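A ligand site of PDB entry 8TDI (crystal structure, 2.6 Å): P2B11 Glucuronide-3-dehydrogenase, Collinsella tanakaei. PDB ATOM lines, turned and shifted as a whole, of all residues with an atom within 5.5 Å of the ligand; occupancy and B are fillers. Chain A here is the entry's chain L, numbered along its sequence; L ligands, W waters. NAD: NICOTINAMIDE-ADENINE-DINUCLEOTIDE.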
ATOM      1  N   ILE A   9     -32.068  35.780   8.246  1.00  0.00           N
ATOM      2  CA  ILE A   9     -30.698  36.138   8.580  1.00  0.00           C
ATOM      3  C   ILE A   9     -29.869  34.933   8.203  1.00  0.00           C
ATOM      4  O   ILE A   9     -30.114  33.867   8.728  1.00  0.00           O
ATOM      5  CB  ILE A   9     -30.568  36.457  10.086  1.00  0.00           C
ATOM      6  CG1 ILE A   9     -31.691  37.353  10.565  1.00  0.00           C
ATOM      7  CG2 ILE A   9     -29.207  37.051  10.416  1.00  0.00           C
ATOM      8  CD1 ILE A   9     -31.849  37.293  12.065  1.00  0.00           C
ATOM      9  N   GLY A  10     -28.927  35.115   7.272  1.00  0.00           N
ATOM     10  CA  GLY A  10     -28.158  33.995   6.755  1.00  0.00           C
ATOM     11  C   GLY A  10     -28.856  33.388   5.553  1.00  0.00           C
ATOM     12  O   GLY A  10     -29.632  32.447   5.700  1.00  0.00           O
ATOM     13  N   VAL A  11     -28.619  33.944   4.374  1.00  0.00           N
ATOM     14  CA  VAL A  11     -29.154  33.329   3.153  1.00  0.00           C
ATOM     15  C   VAL A  11     -28.156  32.269   2.695  1.00  0.00           C
ATOM     16  O   VAL A  11     -27.578  32.364   1.630  1.00  0.00           O
ATOM     17  CB  VAL A  11     -29.428  34.379   2.047  1.00  0.00           C
ATOM     18  CG1 VAL A  11     -30.584  33.939   1.148  1.00  0.00           C
ATOM     19  CG2 VAL A  11     -29.681  35.766   2.635  1.00  0.00           C
ATOM     20  N   GLY A  12     -27.988  31.239   3.540  1.00  0.00           N
ATOM     21  CA  GLY A  12     -27.164  30.073   3.287  1.00  0.00           C
ATOM     22  C   GLY A  12     -28.014  28.990   2.647  1.00  0.00           C
ATOM     23  O   GLY A  12     -29.086  29.316   2.112  1.00  0.00           O
ATOM     24  N   ASN A  13     -27.614  27.739   2.704  1.00  0.00           N
ATOM     25  CA  ASN A  13     -28.454  26.700   2.104  1.00  0.00           C
ATOM     26  C   ASN A  13     -29.853  26.723   2.722  1.00  0.00           C
ATOM     27  O   ASN A  13     -30.833  26.710   1.992  1.00  0.00           O
ATOM     28  CB  ASN A  13     -27.872  25.307   2.273  1.00  0.00           C
ATOM     29  CG  ASN A  13     -26.419  25.255   1.905  1.00  0.00           C
ATOM     30  OD1 ASN A  13     -26.078  25.259   0.711  1.00  0.00           O
ATOM     31  ND2 ASN A  13     -25.540  25.318   2.906  1.00  0.00           N
ATOM     32  N   GLN A  14     -29.950  26.764   4.056  1.00  0.00           N
ATOM     33  CA  GLN A  14     -31.267  26.804   4.665  1.00  0.00           C
ATOM     34  C   GLN A  14     -32.001  28.113   4.368  1.00  0.00           C
ATOM     35  O   GLN A  14     -33.201  28.099   4.052  1.00  0.00           O
ATOM     36  CB  GLN A  14     -31.231  26.460   6.160  1.00  0.00           C
ATOM     37  CG  GLN A  14     -32.550  25.939   6.711  1.00  0.00           C
ATOM     38  CD  GLN A  14     -33.015  24.638   6.079  1.00  0.00           C
ATOM     39  OE1 GLN A  14     -32.351  24.047   5.222  1.00  0.00           O
ATOM     40  NE2 GLN A  14     -34.166  24.169   6.492  1.00  0.00           N
ATOM     41  N   GLY A  15     -31.279  29.232   4.466  1.00  0.00           N
ATOM     42  CA  GLY A  15     -31.890  30.541   4.230  1.00  0.00           C
ATOM     43  C   GLY A  15     -32.410  30.667   2.806  1.00  0.00           C
ATOM     44  O   GLY A  15     -33.502  31.185   2.590  1.00  0.00           O
ATOM     45  N   TYR A  18     -35.594  28.719   2.343  1.00  0.00           N
ATOM     46  CA  TYR A  18     -36.731  29.403   2.929  1.00  0.00           C
ATOM     47  C   TYR A  18     -37.174  30.524   2.002  1.00  0.00           C
ATOM     48  O   TYR A  18     -38.368  30.715   1.765  1.00  0.00           O
ATOM     49  CB  TYR A  18     -36.316  29.911   4.304  1.00  0.00           C
ATOM     50  CG  TYR A  18     -36.153  28.821   5.352  1.00  0.00           C
ATOM     51  CD1 TYR A  18     -36.448  27.489   5.066  1.00  0.00           C
ATOM     52  CD2 TYR A  18     -35.732  29.125   6.643  1.00  0.00           C
ATOM     53  CE1 TYR A  18     -36.270  26.496   6.002  1.00  0.00           C
ATOM     54  CE2 TYR A  18     -35.572  28.143   7.591  1.00  0.00           C
ATOM     55  CZ  TYR A  18     -35.833  26.823   7.278  1.00  0.00           C
ATOM     56  OH  TYR A  18     -35.674  25.858   8.225  1.00  0.00           O
ATOM     57  N   CYS A  46     -30.923  39.046   4.810  1.00  0.00           N
ATOM     58  CA  CYS A  46     -29.724  39.579   5.458  1.00  0.00           C
ATOM     59  C   CYS A  46     -28.581  38.570   5.365  1.00  0.00           C
ATOM     60  O   CYS A  46     -28.749  37.430   5.782  1.00  0.00           O
ATOM     61  CB  CYS A  46     -29.970  39.911   6.927  1.00  0.00           C
ATOM     62  SG  CYS A  46     -28.444  40.176   7.874  1.00  0.00           S
ATOM     63  N   ASP A  47     -27.407  38.999   4.865  1.00  0.00           N
ATOM     64  CA  ASP A  47     -26.219  38.171   4.913  1.00  0.00           C
ATOM     65  C   ASP A  47     -24.981  39.068   4.983  1.00  0.00           C
ATOM     66  O   ASP A  47     -24.973  40.153   4.385  1.00  0.00           O
ATOM     67  CB  ASP A  47     -26.144  37.196   3.738  1.00  0.00           C
ATOM     68  CG  ASP A  47     -25.373  35.922   4.001  1.00  0.00           C
ATOM     69  OD1 ASP A  47     -24.138  35.996   4.244  1.00  0.00           O
ATOM     70  OD2 ASP A  47     -26.012  34.845   3.999  1.00  0.00           O
ATOM     71  N   ILE A  48     -23.943  38.607   5.688  1.00  0.00           N
ATOM     72  CA  ILE A  48     -22.707  39.373   5.795  1.00  0.00           C
ATOM     73  C   ILE A  48     -21.795  39.097   4.603  1.00  0.00           C
ATOM     74  O   ILE A  48     -20.822  39.810   4.427  1.00  0.00           O
ATOM     75  CB  ILE A  48     -21.975  39.150   7.117  1.00  0.00           C
ATOM     76  CG1 ILE A  48     -21.662  37.648   7.319  1.00  0.00           C
ATOM     77  CG2 ILE A  48     -22.761  39.820   8.271  1.00  0.00           C
ATOM     78  CD1 ILE A  48     -20.896  37.246   8.551  1.00  0.00           C
ATOM     79  N   ASP A  49     -22.056  38.026   3.838  1.00  0.00           N
ATOM     80  CA  ASP A  49     -21.209  37.674   2.703  1.00  0.00           C
ATOM     81  C   ASP A  49     -21.633  38.490   1.480  1.00  0.00           C
ATOM     82  O   ASP A  49     -22.803  38.515   1.115  1.00  0.00           O
ATOM     83  CB  ASP A  49     -21.236  36.190   2.445  1.00  0.00           C
ATOM     84  CG  ASP A  49     -20.514  35.648   1.212  1.00  0.00           C
ATOM     85  OD1 ASP A  49     -19.903  36.354   0.377  1.00  0.00           O
ATOM     86  OD2 ASP A  49     -20.702  34.467   0.982  1.00  0.00           O
ATOM     87  N   LYS A  52     -23.375  36.512  -1.334  1.00  0.00           N
ATOM     88  CA  LYS A  52     -24.761  36.234  -1.028  1.00  0.00           C
ATOM     89  C   LYS A  52     -25.632  37.443  -1.359  1.00  0.00           C
ATOM     90  O   LYS A  52     -26.724  37.286  -1.903  1.00  0.00           O
ATOM     91  CB  LYS A  52     -24.897  35.795   0.444  1.00  0.00           C
ATOM     92  CG  LYS A  52     -24.317  34.432   0.760  1.00  0.00           C
ATOM     93  CD  LYS A  52     -24.756  33.317  -0.188  1.00  0.00           C
ATOM     94  CE  LYS A  52     -24.430  31.933   0.085  1.00  0.00           C
ATOM     95  NZ  LYS A  52     -23.553  31.734   1.233  1.00  0.00           N
ATOM     96  N   LYS A  67     -26.993  44.050   5.333  1.00  0.00           N
ATOM     97  CA  LYS A  67     -25.772  43.391   5.799  1.00  0.00           C
ATOM     98  C   LYS A  67     -25.897  43.071   7.284  1.00  0.00           C
ATOM     99  O   LYS A  67     -25.514  41.994   7.732  1.00  0.00           O
ATOM    100  CB  LYS A  67     -24.527  44.244   5.530  1.00  0.00           C
ATOM    101  CG  LYS A  67     -24.342  44.653   4.080  1.00  0.00           C
ATOM    102  CD  LYS A  67     -22.940  45.128   3.753  1.00  0.00           C
ATOM    103  CE  LYS A  67     -21.798  44.122   3.775  1.00  0.00           C
ATOM    104  NZ  LYS A  67     -22.104  42.816   3.165  1.00  0.00           N
ATOM    105  N   TRP A  69     -28.170  42.413  10.534  1.00  0.00           N
ATOM    106  CA  TRP A  69     -29.498  41.934  10.903  1.00  0.00           C
ATOM    107  C   TRP A  69     -30.184  42.888  11.888  1.00  0.00           C
ATOM    108  O   TRP A  69     -31.407  42.888  11.976  1.00  0.00           O
ATOM    109  CB  TRP A  69     -29.416  40.496  11.435  1.00  0.00           C
ATOM    110  CG  TRP A  69     -28.528  40.309  12.641  1.00  0.00           C
ATOM    111  CD1 TRP A  69     -27.217  39.952  12.666  1.00  0.00           C
ATOM    112  CD2 TRP A  69     -28.927  40.500  14.007  1.00  0.00           C
ATOM    113  NE1 TRP A  69     -26.766  39.900  13.964  1.00  0.00           N
ATOM    114  CE2 TRP A  69     -27.788  40.228  14.807  1.00  0.00           C
ATOM    115  CE3 TRP A  69     -30.133  40.862  14.625  1.00  0.00           C
ATOM    116  CZ2 TRP A  69     -27.836  40.306  16.200  1.00  0.00           C
ATOM    117  CZ3 TRP A  69     -30.172  40.950  16.003  1.00  0.00           C
ATOM    118  CH2 TRP A  69     -29.034  40.670  16.768  1.00  0.00           C
ATOM    119  N   THR A  83     -33.407  32.532  12.140  1.00  0.00           N
ATOM    120  CA  THR A  83     -31.967  32.614  12.387  1.00  0.00           C
ATOM    121  C   THR A  83     -31.221  31.520  11.638  1.00  0.00           C
ATOM    122  O   THR A  83     -30.579  30.678  12.256  1.00  0.00           O
ATOM    123  CB  THR A  83     -31.696  32.583  13.888  1.00  0.00           C
ATOM    124  OG1 THR A  83     -31.895  31.257  14.393  1.00  0.00           O
ATOM    125  CG2 THR A  83     -32.590  33.535  14.662  1.00  0.00           C
ATOM    126  N   THR A  84     -31.223  31.606  10.300  1.00  0.00           N
ATOM    127  CA  THR A  84     -30.517  30.642   9.474  1.00  0.00           C
ATOM    128  C   THR A  84     -29.049  31.023   9.367  1.00  0.00           C
ATOM    129  O   THR A  84     -28.519  31.188   8.272  1.00  0.00           O
ATOM    130  CB  THR A  84     -31.196  30.518   8.111  1.00  0.00           C
ATOM    131  OG1 THR A  84     -31.478  31.830   7.626  1.00  0.00           O
ATOM    132  CG2 THR A  84     -32.482  29.728   8.179  1.00  0.00           C
ATOM    133  N   VAL A  85     -28.386  31.096  10.526  1.00  0.00           N
ATOM    134  CA  VAL A  85     -26.974  31.416  10.646  1.00  0.00           C
ATOM    135  C   VAL A  85     -26.319  30.389  11.564  1.00  0.00           C
ATOM    136  O   VAL A  85     -27.015  29.691  12.285  1.00  0.00           O
ATOM    137  CB  VAL A  85     -26.762  32.827  11.211  1.00  0.00           C
ATOM    138  CG1 VAL A  85     -26.943  33.912  10.176  1.00  0.00           C
ATOM    139  CG2 VAL A  85     -27.663  33.105  12.411  1.00  0.00           C
ATOM    140  N   PRO A  86     -24.972  30.292  11.602  1.00  0.00           N
ATOM    141  CA  PRO A  86     -24.297  29.352  12.501  1.00  0.00           C
ATOM    142  C   PRO A  86     -24.864  29.472  13.921  1.00  0.00           C
ATOM    143  O   PRO A  86     -25.348  30.534  14.327  1.00  0.00           O
ATOM    144  CB  PRO A  86     -22.839  29.798  12.410  1.00  0.00           C
ATOM    145  CG  PRO A  86     -22.724  30.291  10.982  1.00  0.00           C
ATOM    146  CD  PRO A  86     -24.032  31.056  10.771  1.00  0.00           C
ATOM    147  N   HIS A  87     -24.766  28.359  14.659  1.00  0.00           N
ATOM    148  CA  HIS A  87     -25.603  28.133  15.831  1.00  0.00           C
ATOM    149  C   HIS A  87     -25.208  29.113  16.942  1.00  0.00           C
ATOM    150  O   HIS A  87     -26.044  29.509  17.755  1.00  0.00           O
ATOM    151  CB  HIS A  87     -25.473  26.681  16.297  1.00  0.00           C
ATOM    152  CG  HIS A  87     -25.499  25.653  15.202  1.00  0.00           C
ATOM    153  ND1 HIS A  87     -24.658  24.555  15.209  1.00  0.00           N
ATOM    154  CD2 HIS A  87     -26.231  25.573  14.080  1.00  0.00           C
ATOM    155  CE1 HIS A  87     -24.885  23.839  14.123  1.00  0.00           C
ATOM    156  NE2 HIS A  87     -25.850  24.437  13.414  1.00  0.00           N
ATOM    157  N   LEU A  89     -24.733  32.133  16.922  1.00  0.00           N
ATOM    158  CA  LEU A  89     -25.451  33.403  16.857  1.00  0.00           C
ATOM    159  C   LEU A  89     -26.912  33.279  17.280  1.00  0.00           C
ATOM    160  O   LEU A  89     -27.574  34.304  17.451  1.00  0.00           O
ATOM    161  CB  LEU A  89     -25.373  33.992  15.440  1.00  0.00           C
ATOM    162  CG  LEU A  89     -23.964  34.237  14.896  1.00  0.00           C
ATOM    163  CD1 LEU A  89     -24.077  35.019  13.583  1.00  0.00           C
ATOM    164  CD2 LEU A  89     -23.036  34.972  15.846  1.00  0.00           C
ATOM    165  N   HIS A  90     -27.435  32.060  17.435  1.00  0.00           N
ATOM    166  CA  HIS A  90     -28.877  31.904  17.577  1.00  0.00           C
ATOM    167  C   HIS A  90     -29.397  32.678  18.790  1.00  0.00           C
ATOM    168  O   HIS A  90     -30.290  33.507  18.655  1.00  0.00           O
ATOM    169  CB  HIS A  90     -29.279  30.436  17.640  1.00  0.00           C
ATOM    170  CG  HIS A  90     -29.149  29.682  16.361  1.00  0.00           C
ATOM    171  ND1 HIS A  90     -29.518  28.358  16.303  1.00  0.00           N
ATOM    172  CD2 HIS A  90     -28.668  29.990  15.137  1.00  0.00           C
ATOM    173  CE1 HIS A  90     -29.292  27.894  15.083  1.00  0.00           C
ATOM    174  NE2 HIS A  90     -28.777  28.876  14.361  1.00  0.00           N
ATOM    175  N   GLU A 107     -33.564  28.791  14.669  1.00  0.00           N
ATOM    176  CA  GLU A 107     -33.258  27.536  14.019  1.00  0.00           C
ATOM    177  C   GLU A 107     -32.767  26.511  15.022  1.00  0.00           C
ATOM    178  O   GLU A 107     -32.362  26.846  16.131  1.00  0.00           O
ATOM    179  CB  GLU A 107     -32.177  27.664  12.949  1.00  0.00           C
ATOM    180  CG  GLU A 107     -32.756  27.892  11.555  1.00  0.00           C
ATOM    181  CD  GLU A 107     -33.667  26.766  11.083  1.00  0.00           C
ATOM    182  OE1 GLU A 107     -34.310  26.964  10.035  1.00  0.00           O
ATOM    183  OE2 GLU A 107     -33.723  25.711  11.746  1.00  0.00           O
ATOM    184  N   LYS A 108     -32.799  25.249  14.584  1.00  0.00           N
ATOM    185  CA  LYS A 108     -32.206  24.157  15.316  1.00  0.00           C
ATOM    186  C   LYS A 108     -30.698  24.180  15.053  1.00  0.00           C
ATOM    187  O   LYS A 108     -30.258  24.632  14.000  1.00  0.00           O
ATOM    188  CB  LYS A 108     -32.826  22.845  14.820  1.00  0.00           C
ATOM    189  CG  LYS A 108     -32.483  22.464  13.370  1.00  0.00           C
ATOM    190  CD  LYS A 108     -31.305  21.523  13.240  1.00  0.00           C
ATOM    191  CE  LYS A 108     -31.013  21.091  11.846  1.00  0.00           C
ATOM    192  NZ  LYS A 108     -30.004  20.039  11.780  1.00  0.00           N
ATOM    193  N   PRO A 109     -29.866  23.750  16.022  1.00  0.00           N
ATOM    194  CA  PRO A 109     -30.296  23.564  17.413  1.00  0.00           C
ATOM    195  C   PRO A 109     -30.477  24.958  18.021  1.00  0.00           C
ATOM    196  O   PRO A 109     -29.911  25.921  17.526  1.00  0.00           O
ATOM    197  CB  PRO A 109     -29.105  22.811  18.026  1.00  0.00           C
ATOM    198  CG  PRO A 109     -27.912  23.305  17.238  1.00  0.00           C
ATOM    199  CD  PRO A 109     -28.423  23.484  15.818  1.00  0.00           C
ATOM    200  N   MET A 135     -37.566  26.015  15.074  1.00  0.00           N
ATOM    201  CA  MET A 135     -37.843  25.318  13.832  1.00  0.00           C
ATOM    202  C   MET A 135     -37.625  23.816  14.032  1.00  0.00           C
ATOM    203  O   MET A 135     -36.658  23.221  13.524  1.00  0.00           O
ATOM    204  CB  MET A 135     -36.938  25.867  12.729  1.00  0.00           C
ATOM    205  CG  MET A 135     -37.179  25.237  11.350  1.00  0.00           C
ATOM    206  SD  MET A 135     -38.818  25.566  10.670  1.00  0.00           S
ATOM    207  CE  MET A 135     -38.421  27.046   9.745  1.00  0.00           C
ATOM    208  N   ASN A 137     -39.073  21.207  12.730  1.00  0.00           N
ATOM    209  CA  ASN A 137     -39.986  21.038  11.598  1.00  0.00           C
ATOM    210  C   ASN A 137     -40.489  19.605  11.528  1.00  0.00           C
ATOM    211  O   ASN A 137     -41.547  19.328  10.981  1.00  0.00           O
ATOM    212  CB  ASN A 137     -39.333  21.538  10.318  1.00  0.00           C
ATOM    213  CG  ASN A 137     -37.951  20.961  10.131  1.00  0.00           C
ATOM    214  OD1 ASN A 137     -36.958  21.613  10.481  1.00  0.00           O
ATOM    215  ND2 ASN A 137     -37.855  19.728   9.653  1.00  0.00           N
ATOM    216  N   SER A 179     -17.896  23.220   4.414  1.00  0.00           N
ATOM    217  CA  SER A 179     -18.174  24.404   5.235  1.00  0.00           C
ATOM    218  C   SER A 179     -17.113  24.573   6.317  1.00  0.00           C
ATOM    219  O   SER A 179     -16.874  23.639   7.069  1.00  0.00           O
ATOM    220  CB  SER A 179     -19.565  24.366   5.865  1.00  0.00           C
ATOM    221  OG  SER A 179     -19.564  24.950   7.161  1.00  0.00           O
ATOM    222  N   TRP A 181     -17.380  26.610   9.041  1.00  0.00           N
ATOM    223  CA  TRP A 181     -18.005  26.673  10.368  1.00  0.00           C
ATOM    224  C   TRP A 181     -18.445  25.278  10.871  1.00  0.00           C
ATOM    225  O   TRP A 181     -18.325  24.985  12.063  1.00  0.00           O
ATOM    226  CB  TRP A 181     -19.158  27.696  10.423  1.00  0.00           C
ATOM    227  CG  TRP A 181     -20.452  27.327   9.733  1.00  0.00           C
ATOM    228  CD1 TRP A 181     -20.743  27.465   8.415  1.00  0.00           C
ATOM    229  CD2 TRP A 181     -21.639  26.810  10.367  1.00  0.00           C
ATOM    230  NE1 TRP A 181     -22.026  27.056   8.163  1.00  0.00           N
ATOM    231  CE2 TRP A 181     -22.598  26.646   9.337  1.00  0.00           C
ATOM    232  CE3 TRP A 181     -21.980  26.460  11.671  1.00  0.00           C
ATOM    233  CZ2 TRP A 181     -23.876  26.127   9.592  1.00  0.00           C
ATOM    234  CZ3 TRP A 181     -23.243  25.965  11.926  1.00  0.00           C
ATOM    235  CH2 TRP A 181     -24.174  25.809  10.891  1.00  0.00           C
ATOM    236  N   ARG A 182     -18.953  24.429   9.960  1.00  0.00           N
ATOM    237  CA  ARG A 182     -19.457  23.120  10.365  1.00  0.00           C
ATOM    238  C   ARG A 182     -18.320  22.207  10.835  1.00  0.00           C
ATOM    239  O   ARG A 182     -17.229  22.322  10.321  1.00  0.00           O
ATOM    240  CB  ARG A 182     -20.296  22.493   9.245  1.00  0.00           C
ATOM    241  CG  ARG A 182     -21.645  23.185   9.092  1.00  0.00           C
ATOM    242  CD  ARG A 182     -22.775  22.219   9.216  1.00  0.00           C
ATOM    243  NE  ARG A 182     -24.084  22.767   8.906  1.00  0.00           N
ATOM    244  CZ  ARG A 182     -25.172  22.770   9.654  1.00  0.00           C
ATOM    245  NH1 ARG A 182     -25.124  22.432  10.921  1.00  0.00           N
ATOM    246  NH2 ARG A 182     -26.293  23.209   9.120  1.00  0.00           N
ATOM    247  N   VAL A 194     -24.577  18.415  16.916  1.00  0.00           N
ATOM    248  CA  VAL A 194     -25.043  19.759  16.626  1.00  0.00           C
ATOM    249  C   VAL A 194     -25.606  19.869  15.193  1.00  0.00           C
ATOM    250  O   VAL A 194     -26.232  20.881  14.870  1.00  0.00           O
ATOM    251  CB  VAL A 194     -23.956  20.833  16.869  1.00  0.00           C
ATOM    252  CG1 VAL A 194     -23.395  20.757  18.285  1.00  0.00           C
ATOM    253  CG2 VAL A 194     -22.838  20.741  15.846  1.00  0.00           C
ATOM    254  N   HIS A 199     -32.711  17.434  15.360  1.00  0.00           N
ATOM    255  CA  HIS A 199     -34.132  17.175  15.142  1.00  0.00           C
ATOM    256  C   HIS A 199     -34.531  15.874  15.841  1.00  0.00           C
ATOM    257  O   HIS A 199     -35.535  15.809  16.543  1.00  0.00           O
ATOM    258  CB  HIS A 199     -34.472  17.116  13.655  1.00  0.00           C
ATOM    259  CG  HIS A 199     -34.717  18.462  13.051  1.00  0.00           C
ATOM    260  ND1 HIS A 199     -35.424  19.448  13.726  1.00  0.00           N
ATOM    261  CD2 HIS A 199     -34.364  18.972  11.850  1.00  0.00           C
ATOM    262  CE1 HIS A 199     -35.475  20.517  12.967  1.00  0.00           C
ATOM    263  NE2 HIS A 199     -34.834  20.249  11.814  1.00  0.00           N
ATOM    264  N   HIS A 328     -41.036  22.759   6.798  1.00  0.00           N
ATOM    265  CA  HIS A 328     -40.542  24.094   7.110  1.00  0.00           C
ATOM    266  C   HIS A 328     -41.650  25.135   6.911  1.00  0.00           C
ATOM    267  O   HIS A 328     -41.846  25.996   7.770  1.00  0.00           O
ATOM    268  CB  HIS A 328     -39.258  24.369   6.332  1.00  0.00           C
ATOM    269  CG  HIS A 328     -38.181  23.382   6.652  1.00  0.00           C
ATOM    270  ND1 HIS A 328     -37.907  22.292   5.845  1.00  0.00           N
ATOM    271  CD2 HIS A 328     -37.349  23.300   7.695  1.00  0.00           C
ATOM    272  CE1 HIS A 328     -36.929  21.584   6.406  1.00  0.00           C
ATOM    273  NE2 HIS A 328     -36.559  22.189   7.506  1.00  0.00           N
HETATM  274  PA  NAD L   1     -24.701  28.026   5.755  1.00  0.00           P
HETATM  275  O1A NAD L   1     -23.280  28.157   6.267  1.00  0.00           O
HETATM  276  O2A NAD L   1     -24.965  27.533   4.371  1.00  0.00           O
HETATM  277  O5B NAD L   1     -25.522  29.412   5.927  1.00  0.00           O
HETATM  278  C5B NAD L   1     -25.265  30.448   6.915  1.00  0.00           C
HETATM  279  C4B NAD L   1     -25.296  31.802   6.237  1.00  0.00           C
HETATM  280  O4B NAD L   1     -25.312  32.822   7.258  1.00  0.00           O
HETATM  281  C3B NAD L   1     -24.101  32.154   5.324  1.00  0.00           C
HETATM  282  O3B NAD L   1     -24.534  32.826   4.139  1.00  0.00           O
HETATM  283  C2B NAD L   1     -23.247  33.098   6.181  1.00  0.00           C
HETATM  284  O2B NAD L   1     -22.464  34.008   5.425  1.00  0.00           O
HETATM  285  C1B NAD L   1     -24.372  33.809   6.895  1.00  0.00           C
HETATM  286  N9A NAD L   1     -23.995  34.528   8.101  1.00  0.00           N
HETATM  287  C8A NAD L   1     -23.055  34.255   9.062  1.00  0.00           C
HETATM  288  N7A NAD L   1     -22.995  35.170  10.005  1.00  0.00           N
HETATM  289  C5A NAD L   1     -23.964  36.090   9.628  1.00  0.00           C
HETATM  290  C6A NAD L   1     -24.404  37.302  10.204  1.00  0.00           C
HETATM  291  N6A NAD L   1     -23.884  37.808  11.319  1.00  0.00           N
HETATM  292  N1A NAD L   1     -25.386  37.986   9.566  1.00  0.00           N
HETATM  293  C2A NAD L   1     -25.883  37.490   8.418  1.00  0.00           C
HETATM  294  N3A NAD L   1     -25.559  36.365   7.782  1.00  0.00           N
HETATM  295  C4A NAD L   1     -24.591  35.706   8.460  1.00  0.00           C
HETATM  296  O3  NAD L   1     -25.471  27.038   6.767  1.00  0.00           O
HETATM  297  PN  NAD L   1     -26.968  26.416   6.796  1.00  0.00           P
HETATM  298  O1N NAD L   1     -26.908  24.990   6.329  1.00  0.00           O
HETATM  299  O2N NAD L   1     -27.941  27.334   6.092  1.00  0.00           O
HETATM  300  O5D NAD L   1     -27.233  26.414   8.388  1.00  0.00           O
HETATM  301  C5D NAD L   1     -27.422  27.618   9.166  1.00  0.00           C
HETATM  302  C4D NAD L   1     -28.440  27.344  10.246  1.00  0.00           C
HETATM  303  O4D NAD L   1     -29.604  26.708   9.666  1.00  0.00           O
HETATM  304  C3D NAD L   1     -27.947  26.427  11.376  1.00  0.00           C
HETATM  305  O3D NAD L   1     -28.477  26.787  12.639  1.00  0.00           O
HETATM  306  C2D NAD L   1     -28.514  25.068  10.974  1.00  0.00           C
HETATM  307  O2D NAD L   1     -28.655  24.281  12.144  1.00  0.00           O
HETATM  308  C1D NAD L   1     -29.854  25.499  10.372  1.00  0.00           C
HETATM  309  N1N NAD L   1     -30.433  24.494   9.466  1.00  0.00           N
HETATM  310  C2N NAD L   1     -31.678  23.998   9.758  1.00  0.00           C
HETATM  311  C3N NAD L   1     -32.204  22.972   8.980  1.00  0.00           C
HETATM  312  C7N NAD L   1     -33.590  22.503   9.307  1.00  0.00           C
HETATM  313  O7N NAD L   1     -34.077  21.555   8.670  1.00  0.00           O
HETATM  314  N7N NAD L   1     -34.271  23.181  10.235  1.00  0.00           N
HETATM  315  C4N NAD L   1     -31.486  22.476   7.893  1.00  0.00           C
HETATM  316  C5N NAD L   1     -30.230  22.975   7.623  1.00  0.00           C
HETATM  317  C6N NAD L   1     -29.707  23.978   8.410  1.00  0.00           C
HETATM  318  O   HOH W   1     -28.272  23.499   4.710  1.00  0.00           O
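The backbone carbonyl oxygen (O) of Lys 108 sits at hydrogen-bond distance from an oxygen (O2D) of the ligand, at 2.5 Å.
The side-chain carboxylate (OD2) of Asp 47 is in hydrogen-bond range of an oxygen (O3B) of the ligand, at 2.5 Å.
The indole nitrogen (NE1) of Trp 181 lies within hydrogen-bond range of an oxygen (O1A) of the ligand.
The backbone NH (N) of Asn 13 is in hydrogen-bond range of an oxygen (O2A) of the ligand.
The side-chain amide nitrogen (ND2) of Asn 13 sits at hydrogen-bond distance from an oxygen (O2A) of the ligand (2.7 Å).
An oxygen (O3D) of the ligand is in hydrogen-bond range of a ring nitrogen (NE2) of His 90 (2.7 Å).
A ring nitrogen (NE2) of His 328 lies within hydrogen-bond range of an oxygen (O7N) of the ligand (2.8 Å).
N of Gln 14 sits at hydrogen-bond distance from O2N of the ligand, 2.9 Å away.
The side-chain amide nitrogen (NE2) of Gln 14 lies close to an oxygen (O7N) of the ligand (3.4 Å).
A ring nitrogen (NE2) of His 87 sits at hydrogen-bond distance from an oxygen (O2D) of the ligand (3.1 Å).
A nitrogen (N7N) of the ligand is in hydrogen-bond range of the side-chain carboxylate (OE2) of Glu 107, at 3.0 Å.
A nitrogen (N7N) of the ligand sits at hydrogen-bond distance from the side-chain amide oxygen of Asn 137 (3.1 Å).
An oxygen (O3B) of the ligand lies within hydrogen-bond range of the side-chain amino group of Lys 52.
The backbone carbonyl oxygen of Val 85 is in hydrogen-bond range of an oxygen (O3D) of the ligand (3.3 Å).
The backbone NH (N) of Ile 48 lies within hydrogen-bond range of a nitrogen (N3A) of the ligand (3.5 Å).
The guanidinium group (NH2) of Arg 182 is in salt-bridge range of an oxygen (O1N) of the ligand (3.4 Å).
N7N of the ligand is in hydrogen-bond range of NE2 of His 199 (3.4 Å).
Merely in contact with the ligand: Ile 9 (3.9 Å), Gly 10 (3.1 Å), Val 11 (3.9 Å), Gly 12 (3.2 Å), Tyr 18 (3.6 Å), Cys 46 (3.8 Å), Asp 49 (3.9 Å), Thr 84 (3.6 Å), Pro 86 (3.8 Å), Leu 89 (3.6 Å), Pro 109 (3.8 Å) and Met 135 (3.7 Å).
Of the 33 residues printed, 27 come within 4 Å of the ligand.
The nearest printed residue that does not touch the ligand is Trp 69 (4.1 Å).
A ring nitrogen (NE2) of His 90 sits at hydrogen-bond distance from the backbone carbonyl oxygen (O) of Val 85, 2.8 Å away.
A ring nitrogen (ND1) of His 90 is in hydrogen-bond range of the backbone carbonyl oxygen (O) of Pro 109, 2.8 Å away.
The side-chain amide nitrogen of Gln 14 is in hydrogen-bond range of the side-chain hydroxyl of Tyr 18 (2.9 Å).
The backbone NH of Glu 107 lies within hydrogen-bond range of the side-chain hydroxyl of Thr 83 (3.0 Å).
OG1 of Thr 84 is in hydrogen-bond range of O of Gly 10 (2.7 Å).
The backbone NH (N) of Arg 182 lies within hydrogen-bond range of the side-chain hydroxyl (OG) of Ser 179 (2.9 Å).
SG of Cys 46 sits at hydrogen-bond distance from N of Trp 69, at 3.5 Å.
O of Lys 67 sits at hydrogen-bond distance from SG of Cys 46 (3.5 Å).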
